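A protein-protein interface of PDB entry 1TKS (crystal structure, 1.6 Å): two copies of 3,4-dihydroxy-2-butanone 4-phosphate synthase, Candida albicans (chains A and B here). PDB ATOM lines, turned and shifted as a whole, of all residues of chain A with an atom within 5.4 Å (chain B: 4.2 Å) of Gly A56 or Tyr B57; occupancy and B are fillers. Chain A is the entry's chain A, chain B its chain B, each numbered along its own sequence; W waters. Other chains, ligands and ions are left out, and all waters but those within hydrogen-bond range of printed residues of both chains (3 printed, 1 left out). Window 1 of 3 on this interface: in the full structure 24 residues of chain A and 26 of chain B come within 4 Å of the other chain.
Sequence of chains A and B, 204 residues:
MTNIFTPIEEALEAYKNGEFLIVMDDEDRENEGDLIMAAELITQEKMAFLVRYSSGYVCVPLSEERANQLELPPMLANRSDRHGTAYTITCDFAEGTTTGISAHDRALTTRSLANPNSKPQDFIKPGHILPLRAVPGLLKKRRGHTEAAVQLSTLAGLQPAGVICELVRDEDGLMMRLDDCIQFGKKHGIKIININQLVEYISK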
ATOM      1  N   VAL A  51     -18.814  18.932   2.325  1.00  0.00           N
ATOM      2  CA  VAL A  51     -19.246  19.520   1.062  1.00  0.00           C
ATOM      3  C   VAL A  51     -20.612  18.983   0.646  1.00  0.00           C
ATOM      4  O   VAL A  51     -21.473  19.738   0.199  1.00  0.00           O
ATOM      5  CB  VAL A  51     -18.208  19.244  -0.057  1.00  0.00           C
ATOM      6  CG1 VAL A  51     -18.743  19.699  -1.403  1.00  0.00           C
ATOM      7  CG2 VAL A  51     -16.911  19.979   0.264  1.00  0.00           C
ATOM      8  N   SER A  54     -23.403  20.785   2.701  1.00  0.00           N
ATOM      9  CA  SER A  54     -23.278  22.215   2.941  1.00  0.00           C
ATOM     10  C   SER A  54     -23.303  23.057   1.676  1.00  0.00           C
ATOM     11  O   SER A  54     -23.478  22.546   0.574  1.00  0.00           O
ATOM     12  CB  SER A  54     -21.977  22.496   3.679  1.00  0.00           C
ATOM     13  OG  SER A  54     -20.885  22.301   2.803  1.00  0.00           O
ATOM     14  N   SER A  55     -23.114  24.360   1.857  1.00  0.00           N
ATOM     15  CA  SER A  55     -23.100  25.304   0.745  1.00  0.00           C
ATOM     16  C   SER A  55     -21.882  25.074  -0.140  1.00  0.00           C
ATOM     17  O   SER A  55     -21.850  25.533  -1.280  1.00  0.00           O
ATOM     18  CB  SER A  55     -23.044  26.740   1.264  1.00  0.00           C
ATOM     19  OG  SER A  55     -21.726  27.075   1.653  1.00  0.00           O
ATOM     20  N   GLY A  56     -20.869  24.396   0.399  1.00  0.00           N
ATOM     21  CA  GLY A  56     -19.666  24.146  -0.373  1.00  0.00           C
ATOM     22  C   GLY A  56     -18.665  25.283  -0.316  1.00  0.00           C
ATOM     23  O   GLY A  56     -17.543  25.151  -0.801  1.00  0.00           O
ATOM     24  N   TYR A  57     -19.064  26.403   0.279  1.00  0.00           N
ATOM     25  CA  TYR A  57     -18.183  27.564   0.418  1.00  0.00           C
ATOM     26  C   TYR A  57     -17.436  27.307   1.724  1.00  0.00           C
ATOM     27  O   TYR A  57     -17.646  27.984   2.734  1.00  0.00           O
ATOM     28  CB  TYR A  57     -19.027  28.846   0.503  1.00  0.00           C
ATOM     29  CG  TYR A  57     -18.351  30.110   0.009  1.00  0.00           C
ATOM     30  CD1 TYR A  57     -17.915  30.224  -1.312  1.00  0.00           C
ATOM     31  CD2 TYR A  57     -18.182  31.207   0.856  1.00  0.00           C
ATOM     32  CE1 TYR A  57     -17.326  31.400  -1.777  1.00  0.00           C
ATOM     33  CE2 TYR A  57     -17.594  32.389   0.399  1.00  0.00           C
ATOM     34  CZ  TYR A  57     -17.171  32.478  -0.914  1.00  0.00           C
ATOM     35  OH  TYR A  57     -16.596  33.648  -1.370  1.00  0.00           O
ATOM     36  N   VAL A  58     -16.563  26.303   1.683  1.00  0.00           N
ATOM     37  CA  VAL A  58     -15.799  25.872   2.850  1.00  0.00           C
ATOM     38  C   VAL A  58     -14.734  26.864   3.286  1.00  0.00           C
ATOM     39  O   VAL A  58     -13.850  27.229   2.512  1.00  0.00           O
ATOM     40  CB  VAL A  58     -15.151  24.487   2.594  1.00  0.00           C
ATOM     41  CG1 VAL A  58     -14.431  23.999   3.844  1.00  0.00           C
ATOM     42  CG2 VAL A  58     -16.228  23.476   2.187  1.00  0.00           C
ATOM     43  N   THR A  90      -7.610  33.676  -0.902  1.00  0.00           N
ATOM     44  CA  THR A  90      -7.787  32.226  -0.909  1.00  0.00           C
ATOM     45  C   THR A  90      -6.476  31.500  -1.181  1.00  0.00           C
ATOM     46  O   THR A  90      -5.513  32.100  -1.653  1.00  0.00           O
ATOM     47  CB  THR A  90      -8.842  31.799  -1.946  1.00  0.00           C
ATOM     48  OG1 THR A  90      -8.449  32.254  -3.246  1.00  0.00           O
ATOM     49  CG2 THR A  90     -10.200  32.392  -1.584  1.00  0.00           C
ATOM     50  N   ILE A 101      -9.733  21.896  -5.826  1.00  0.00           N
ATOM     51  CA  ILE A 101     -11.144  21.843  -5.458  1.00  0.00           C
ATOM     52  C   ILE A 101     -11.619  20.473  -4.935  1.00  0.00           C
ATOM     53  O   ILE A 101     -12.605  20.391  -4.203  1.00  0.00           O
ATOM     54  CB  ILE A 101     -12.025  22.280  -6.673  1.00  0.00           C
ATOM     55  CG1 ILE A 101     -13.410  22.728  -6.196  1.00  0.00           C
ATOM     56  CG2 ILE A 101     -12.155  21.153  -7.679  1.00  0.00           C
ATOM     57  CD1 ILE A 101     -13.446  24.171  -5.726  1.00  0.00           C
ATOM     58  N   ARG A 106      -8.878  19.963  -0.824  1.00  0.00           N
ATOM     59  CA  ARG A 106      -9.368  20.919   0.155  1.00  0.00           C
ATOM     60  C   ARG A 106      -9.079  20.444   1.574  1.00  0.00           C
ATOM     61  O   ARG A 106      -8.772  21.256   2.443  1.00  0.00           O
ATOM     62  CB  ARG A 106     -10.863  21.190  -0.044  1.00  0.00           C
ATOM     63  CG  ARG A 106     -11.140  22.047  -1.275  1.00  0.00           C
ATOM     64  CD  ARG A 106     -12.435  22.842  -1.171  1.00  0.00           C
ATOM     65  NE  ARG A 106     -13.577  22.107  -1.702  1.00  0.00           N
ATOM     66  CZ  ARG A 106     -14.812  22.596  -1.775  1.00  0.00           C
ATOM     67  NH1 ARG A 106     -15.077  23.823  -1.346  1.00  0.00           N
ATOM     68  NH2 ARG A 106     -15.784  21.863  -2.304  1.00  0.00           N
ATOM     69  N   GLY A 127      -6.597  30.378  -4.283  1.00  0.00           N
ATOM     70  CA  GLY A 127      -6.837  28.952  -4.263  1.00  0.00           C
ATOM     71  C   GLY A 127      -8.299  28.587  -4.121  1.00  0.00           C
ATOM     72  O   GLY A 127      -9.183  29.356  -4.509  1.00  0.00           O
ATOM     73  N   HIS A 128      -8.558  27.418  -3.544  1.00  0.00           N
ATOM     74  CA  HIS A 128      -9.924  26.940  -3.383  1.00  0.00           C
ATOM     75  C   HIS A 128     -10.406  26.827  -1.939  1.00  0.00           C
ATOM     76  O   HIS A 128     -11.498  26.323  -1.687  1.00  0.00           O
ATOM     77  CB  HIS A 128     -10.087  25.604  -4.117  1.00  0.00           C
ATOM     78  CG  HIS A 128      -9.808  25.695  -5.588  1.00  0.00           C
ATOM     79  ND1 HIS A 128      -8.531  25.774  -6.100  1.00  0.00           N
ATOM     80  CD2 HIS A 128     -10.645  25.767  -6.653  1.00  0.00           C
ATOM     81  CE1 HIS A 128      -8.591  25.892  -7.416  1.00  0.00           C
ATOM     82  NE2 HIS A 128      -9.863  25.891  -7.775  1.00  0.00           N
ATOM     83  N   ILE A 129      -9.586  27.289  -0.997  1.00  0.00           N
ATOM     84  CA  ILE A 129      -9.952  27.300   0.414  1.00  0.00           C
ATOM     85  C   ILE A 129     -10.018  28.760   0.851  1.00  0.00           C
ATOM     86  O   ILE A 129      -9.177  29.573   0.457  1.00  0.00           O
ATOM     87  CB  ILE A 129      -8.928  26.537   1.286  1.00  0.00           C
ATOM     88  CG1 ILE A 129      -9.242  25.044   1.254  1.00  0.00           C
ATOM     89  CG2 ILE A 129      -8.951  27.059   2.723  1.00  0.00           C
ATOM     90  CD1 ILE A 129      -9.226  24.453  -0.137  1.00  0.00           C
ATOM     91  N   LEU A 130     -11.037  29.081   1.644  1.00  0.00           N
ATOM     92  CA  LEU A 130     -11.261  30.438   2.149  1.00  0.00           C
ATOM     93  C   LEU A 130     -10.882  30.592   3.627  1.00  0.00           C
ATOM     94  O   LEU A 130     -11.699  30.320   4.511  1.00  0.00           O
ATOM     95  CB  LEU A 130     -12.745  30.806   1.975  1.00  0.00           C
ATOM     96  CG  LEU A 130     -13.306  30.863   0.545  1.00  0.00           C
ATOM     97  CD1 LEU A 130     -14.621  30.081   0.461  1.00  0.00           C
ATOM     98  CD2 LEU A 130     -13.525  32.316   0.141  1.00  0.00           C
ATOM     99  N   CYS A 165     -18.720  25.266   7.407  1.00  0.00           N
ATOM    100  CA  CYS A 165     -19.586  25.444   6.254  1.00  0.00           C
ATOM    101  C   CYS A 165     -21.034  25.327   6.695  1.00  0.00           C
ATOM    102  O   CYS A 165     -21.345  24.607   7.645  1.00  0.00           O
ATOM    103  CB  CYS A 165     -19.279  24.441   5.146  1.00  0.00           C
ATOM    104  SG  CYS A 165     -19.686  25.136   3.520  1.00  0.00           S
ATOM    105  N   GLU A 166     -21.915  26.042   6.000  1.00  0.00           N
ATOM    106  CA  GLU A 166     -23.343  26.070   6.334  1.00  0.00           C
ATOM    107  C   GLU A 166     -24.135  24.853   5.885  1.00  0.00           C
ATOM    108  O   GLU A 166     -24.056  24.451   4.728  1.00  0.00           O
ATOM    109  CB  GLU A 166     -24.015  27.308   5.719  1.00  0.00           C
ATOM    110  CG  GLU A 166     -23.362  28.641   6.030  1.00  0.00           C
ATOM    111  CD  GLU A 166     -22.227  28.978   5.085  1.00  0.00           C
ATOM    112  OE1 GLU A 166     -21.802  28.098   4.305  1.00  0.00           O
ATOM    113  OE2 GLU A 166     -21.755  30.135   5.126  1.00  0.00           O
ATOM    114  N   SER B  55     -19.357  21.146  -6.080  1.00  0.00           N
ATOM    115  CA  SER B  55     -18.420  21.450  -5.007  1.00  0.00           C
ATOM    116  C   SER B  55     -18.897  22.626  -4.175  1.00  0.00           C
ATOM    117  O   SER B  55     -18.391  22.846  -3.080  1.00  0.00           O
ATOM    118  CB  SER B  55     -17.048  21.804  -5.580  1.00  0.00           C
ATOM    119  OG  SER B  55     -17.053  23.146  -6.059  1.00  0.00           O
ATOM    120  N   GLY B  56     -19.844  23.391  -4.709  1.00  0.00           N
ATOM    121  CA  GLY B  56     -20.352  24.543  -3.987  1.00  0.00           C
ATOM    122  C   GLY B  56     -19.501  25.794  -4.123  1.00  0.00           C
ATOM    123  O   GLY B  56     -19.919  26.872  -3.709  1.00  0.00           O
ATOM    124  N   TYR B  57     -18.303  25.654  -4.687  1.00  0.00           N
ATOM    125  CA  TYR B  57     -17.404  26.791  -4.901  1.00  0.00           C
ATOM    126  C   TYR B  57     -17.900  27.407  -6.208  1.00  0.00           C
ATOM    127  O   TYR B  57     -17.259  27.289  -7.249  1.00  0.00           O
ATOM    128  CB  TYR B  57     -15.958  26.288  -5.053  1.00  0.00           C
ATOM    129  CG  TYR B  57     -14.890  27.274  -4.630  1.00  0.00           C
ATOM    130  CD1 TYR B  57     -14.823  27.729  -3.316  1.00  0.00           C
ATOM    131  CD2 TYR B  57     -13.931  27.734  -5.534  1.00  0.00           C
ATOM    132  CE1 TYR B  57     -13.829  28.615  -2.907  1.00  0.00           C
ATOM    133  CE2 TYR B  57     -12.930  28.624  -5.134  1.00  0.00           C
ATOM    134  CZ  TYR B  57     -12.886  29.057  -3.821  1.00  0.00           C
ATOM    135  OH  TYR B  57     -11.902  29.926  -3.401  1.00  0.00           O
ATOM    136  N   VAL B  58     -19.056  28.063  -6.137  1.00  0.00           N
ATOM    137  CA  VAL B  58     -19.695  28.644  -7.315  1.00  0.00           C
ATOM    138  C   VAL B  58     -19.029  29.902  -7.851  1.00  0.00           C
ATOM    139  O   VAL B  58     -18.882  30.901  -7.142  1.00  0.00           O
ATOM    140  CB  VAL B  58     -21.192  28.924  -7.031  1.00  0.00           C
ATOM    141  CG1 VAL B  58     -21.863  29.514  -8.259  1.00  0.00           C
ATOM    142  CG2 VAL B  58     -21.892  27.620  -6.641  1.00  0.00           C
ATOM    143  N   CYS B  59     -18.646  29.837  -9.123  1.00  0.00           N
ATOM    144  CA  CYS B  59     -17.966  30.932  -9.802  1.00  0.00           C
ATOM    145  C   CYS B  59     -18.804  31.561 -10.905  1.00  0.00           C
ATOM    146  O   CYS B  59     -19.665  30.912 -11.502  1.00  0.00           O
ATOM    147  CB  CYS B  59     -16.641  30.428 -10.376  1.00  0.00           C
ATOM    148  SG  CYS B  59     -15.483  29.812  -9.120  1.00  0.00           S
ATOM    149  N   TYR B  87      -9.045  34.614 -10.403  1.00  0.00           N
ATOM    150  CA  TYR B  87     -10.183  35.024  -9.589  1.00  0.00           C
ATOM    151  C   TYR B  87     -10.123  36.520  -9.323  1.00  0.00           C
ATOM    152  O   TYR B  87      -9.051  37.122  -9.371  1.00  0.00           O
ATOM    153  CB  TYR B  87     -10.162  34.335  -8.224  1.00  0.00           C
ATOM    154  CG  TYR B  87     -10.274  32.835  -8.242  1.00  0.00           C
ATOM    155  CD1 TYR B  87      -9.135  32.033  -8.323  1.00  0.00           C
ATOM    156  CD2 TYR B  87     -11.515  32.214  -8.145  1.00  0.00           C
ATOM    157  CE1 TYR B  87      -9.232  30.647  -8.302  1.00  0.00           C
ATOM    158  CE2 TYR B  87     -11.626  30.832  -8.125  1.00  0.00           C
ATOM    159  CZ  TYR B  87     -10.484  30.054  -8.202  1.00  0.00           C
ATOM    160  OH  TYR B  87     -10.587  28.684  -8.169  1.00  0.00           O
ATOM    161  N   LEU B 130     -17.752  34.056  -6.437  1.00  0.00           N
ATOM    162  CA  LEU B 130     -16.406  34.155  -6.982  1.00  0.00           C
ATOM    163  C   LEU B 130     -16.397  34.505  -8.478  1.00  0.00           C
ATOM    164  O   LEU B 130     -16.452  33.615  -9.329  1.00  0.00           O
ATOM    165  CB  LEU B 130     -15.668  32.821  -6.768  1.00  0.00           C
ATOM    166  CG  LEU B 130     -15.411  32.369  -5.320  1.00  0.00           C
ATOM    167  CD1 LEU B 130     -15.864  30.919  -5.139  1.00  0.00           C
ATOM    168  CD2 LEU B 130     -13.926  32.507  -4.985  1.00  0.00           C
ATOM    169  N   CYS B 165     -19.703  25.399 -11.839  1.00  0.00           N
ATOM    170  CA  CYS B 165     -19.270  24.661 -10.655  1.00  0.00           C
ATOM    171  C   CYS B 165     -19.089  23.196 -11.027  1.00  0.00           C
ATOM    172  O   CYS B 165     -19.798  22.679 -11.888  1.00  0.00           O
ATOM    173  CB  CYS B 165     -20.271  24.810  -9.508  1.00  0.00           C
ATOM    174  SG  CYS B 165     -19.463  24.601  -7.876  1.00  0.00           S
HETATM  175  O   HOH W   1     -10.538  31.816  -4.983  1.00  0.00           O
HETATM  176  O   HOH W   2     -12.735  27.357  -8.928  1.00  0.00           O
HETATM  177  O   HOH W   3     -10.298  26.121 -10.380  1.00  0.00           O
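The guanidinium group of Arg A106 lies within hydrogen-bond range of the backbone carbonyl oxygen of Ser B55 (2.9 Å).
OH of Tyr B57 sits at hydrogen-bond distance from O of Gly A127, 3.0 Å away.
OH of Tyr B87 is in hydrogen-bond range of NE2 of His A128.
O of Gly B56 lies close to O of Ser A55, at 3.4 Å.
O of Gly A56 sits close to O of Ser B55 (3.4 Å).
N of Gly A56 is in hydrogen-bond range of SG of Cys A165 (3.4 Å).
N of Tyr A57 sits at hydrogen-bond distance from SG of Cys A165, 3.5 Å away.
The backbone carbonyl oxygen (O) of Val A58 lies within hydrogen-bond range of the backbone NH (N) of Leu A130 (3.5 Å).
OG1 of Thr A90 sits at hydrogen-bond distance from N of Gly A127.
NE of Arg A106 is in hydrogen-bond range of O of Ile A101, 3.2 Å away.
The backbone carbonyl oxygen (O) of Tyr B57 lies within hydrogen-bond range of the side-chain sulfur (SG) of Cys B165 (3.5 Å).
Among the printed residues, merely in contact across the chains: Val A51 with Ser B55, Gly A56 with Gly B56, Gly A56 with Tyr B57, Tyr A57 with Leu B130, Thr A90 with Tyr B57, Ile A101 with Ser B55, Ile A101 with Tyr B57, Gly A127 with Tyr B87, His A128 with Tyr B57 and Leu A130 with Tyr B57.
Of the printed residues of chain B, Gly A56 touches Ser B55 (3.3 Å), Gly B56 (3.7 Å) and Tyr B57 (3.99 Å).
Of the printed residues of chain B, Tyr A57 touches Leu B130 (3.7 Å).
Val A58 touches none of the printed residues of chain B.
Of the printed residues of chain B, Leu A130 touches Tyr B57 (3.8 Å).
Of the printed residues of chain A, Ser B55 touches Val A51 (3.6 Å), Gly A56 (3.3 Å), Ile A101 (3.7 Å) and Arg A106 (2.9 Å).
Of the printed residues of chain A, Gly B56 touches Ser A55 and Gly A56.
Cys B59 touches none of the printed residues of chain A.
Printed residues of chain A within 4 Å of Tyr B87: Gly A127 and His A128.
The nearest printed residue of chain B that does not touch Gly A56 is Val B58 (6.3 Å).
The nearest printed residue of chain A that does not touch Tyr B57 is Ile A129 (4.3 Å).
The nearest printed residue of chain B that does not touch Arg A106 is Tyr B57 (4.4 Å).
Printed residues of chain B that touch a printed residue of chain A: Ser B55, Gly B56, Tyr B57, Tyr B87 and Leu B130.
Printed residues of chain A that touch a printed residue of chain B: Val A51, Ser A55, Gly A56, Tyr A57, Thr A90, Ile A101, Arg A106, Gly A127, His A128 and Leu A130.
Along chain A the printed residues that touch a printed residue of chain B span positions 51 to 130.
Among the printed residues, 15 pairs touch across the chains.
Ser A55 touches Gly B56, and with the chains exchanged Gly A56 touches Ser B55.
Gly B56 touches its own counterpart, Gly A56.
Gly A56 touches Tyr B57, but with the chains exchanged Tyr A57 does not touch Gly B56 (4.1 Å).
Tyr A57 touches Leu B130, and with the chains exchanged Leu A130 touches Tyr B57.
Water W2 lies within hydrogen-bond range of the side-chain hydroxyl (OH) of Tyr B87, a ring nitrogen (NE2) of His A128 and the side-chain sulfur (SG) of Cys B59.
Water W3 bridges NE2 of His A128 (2.7 Å) and OH of Tyr B87 (3.4 Å).
Water W1 lies within hydrogen-bond range of OG1 of Thr A90, OH of Tyr B57 and O of Gly A127.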
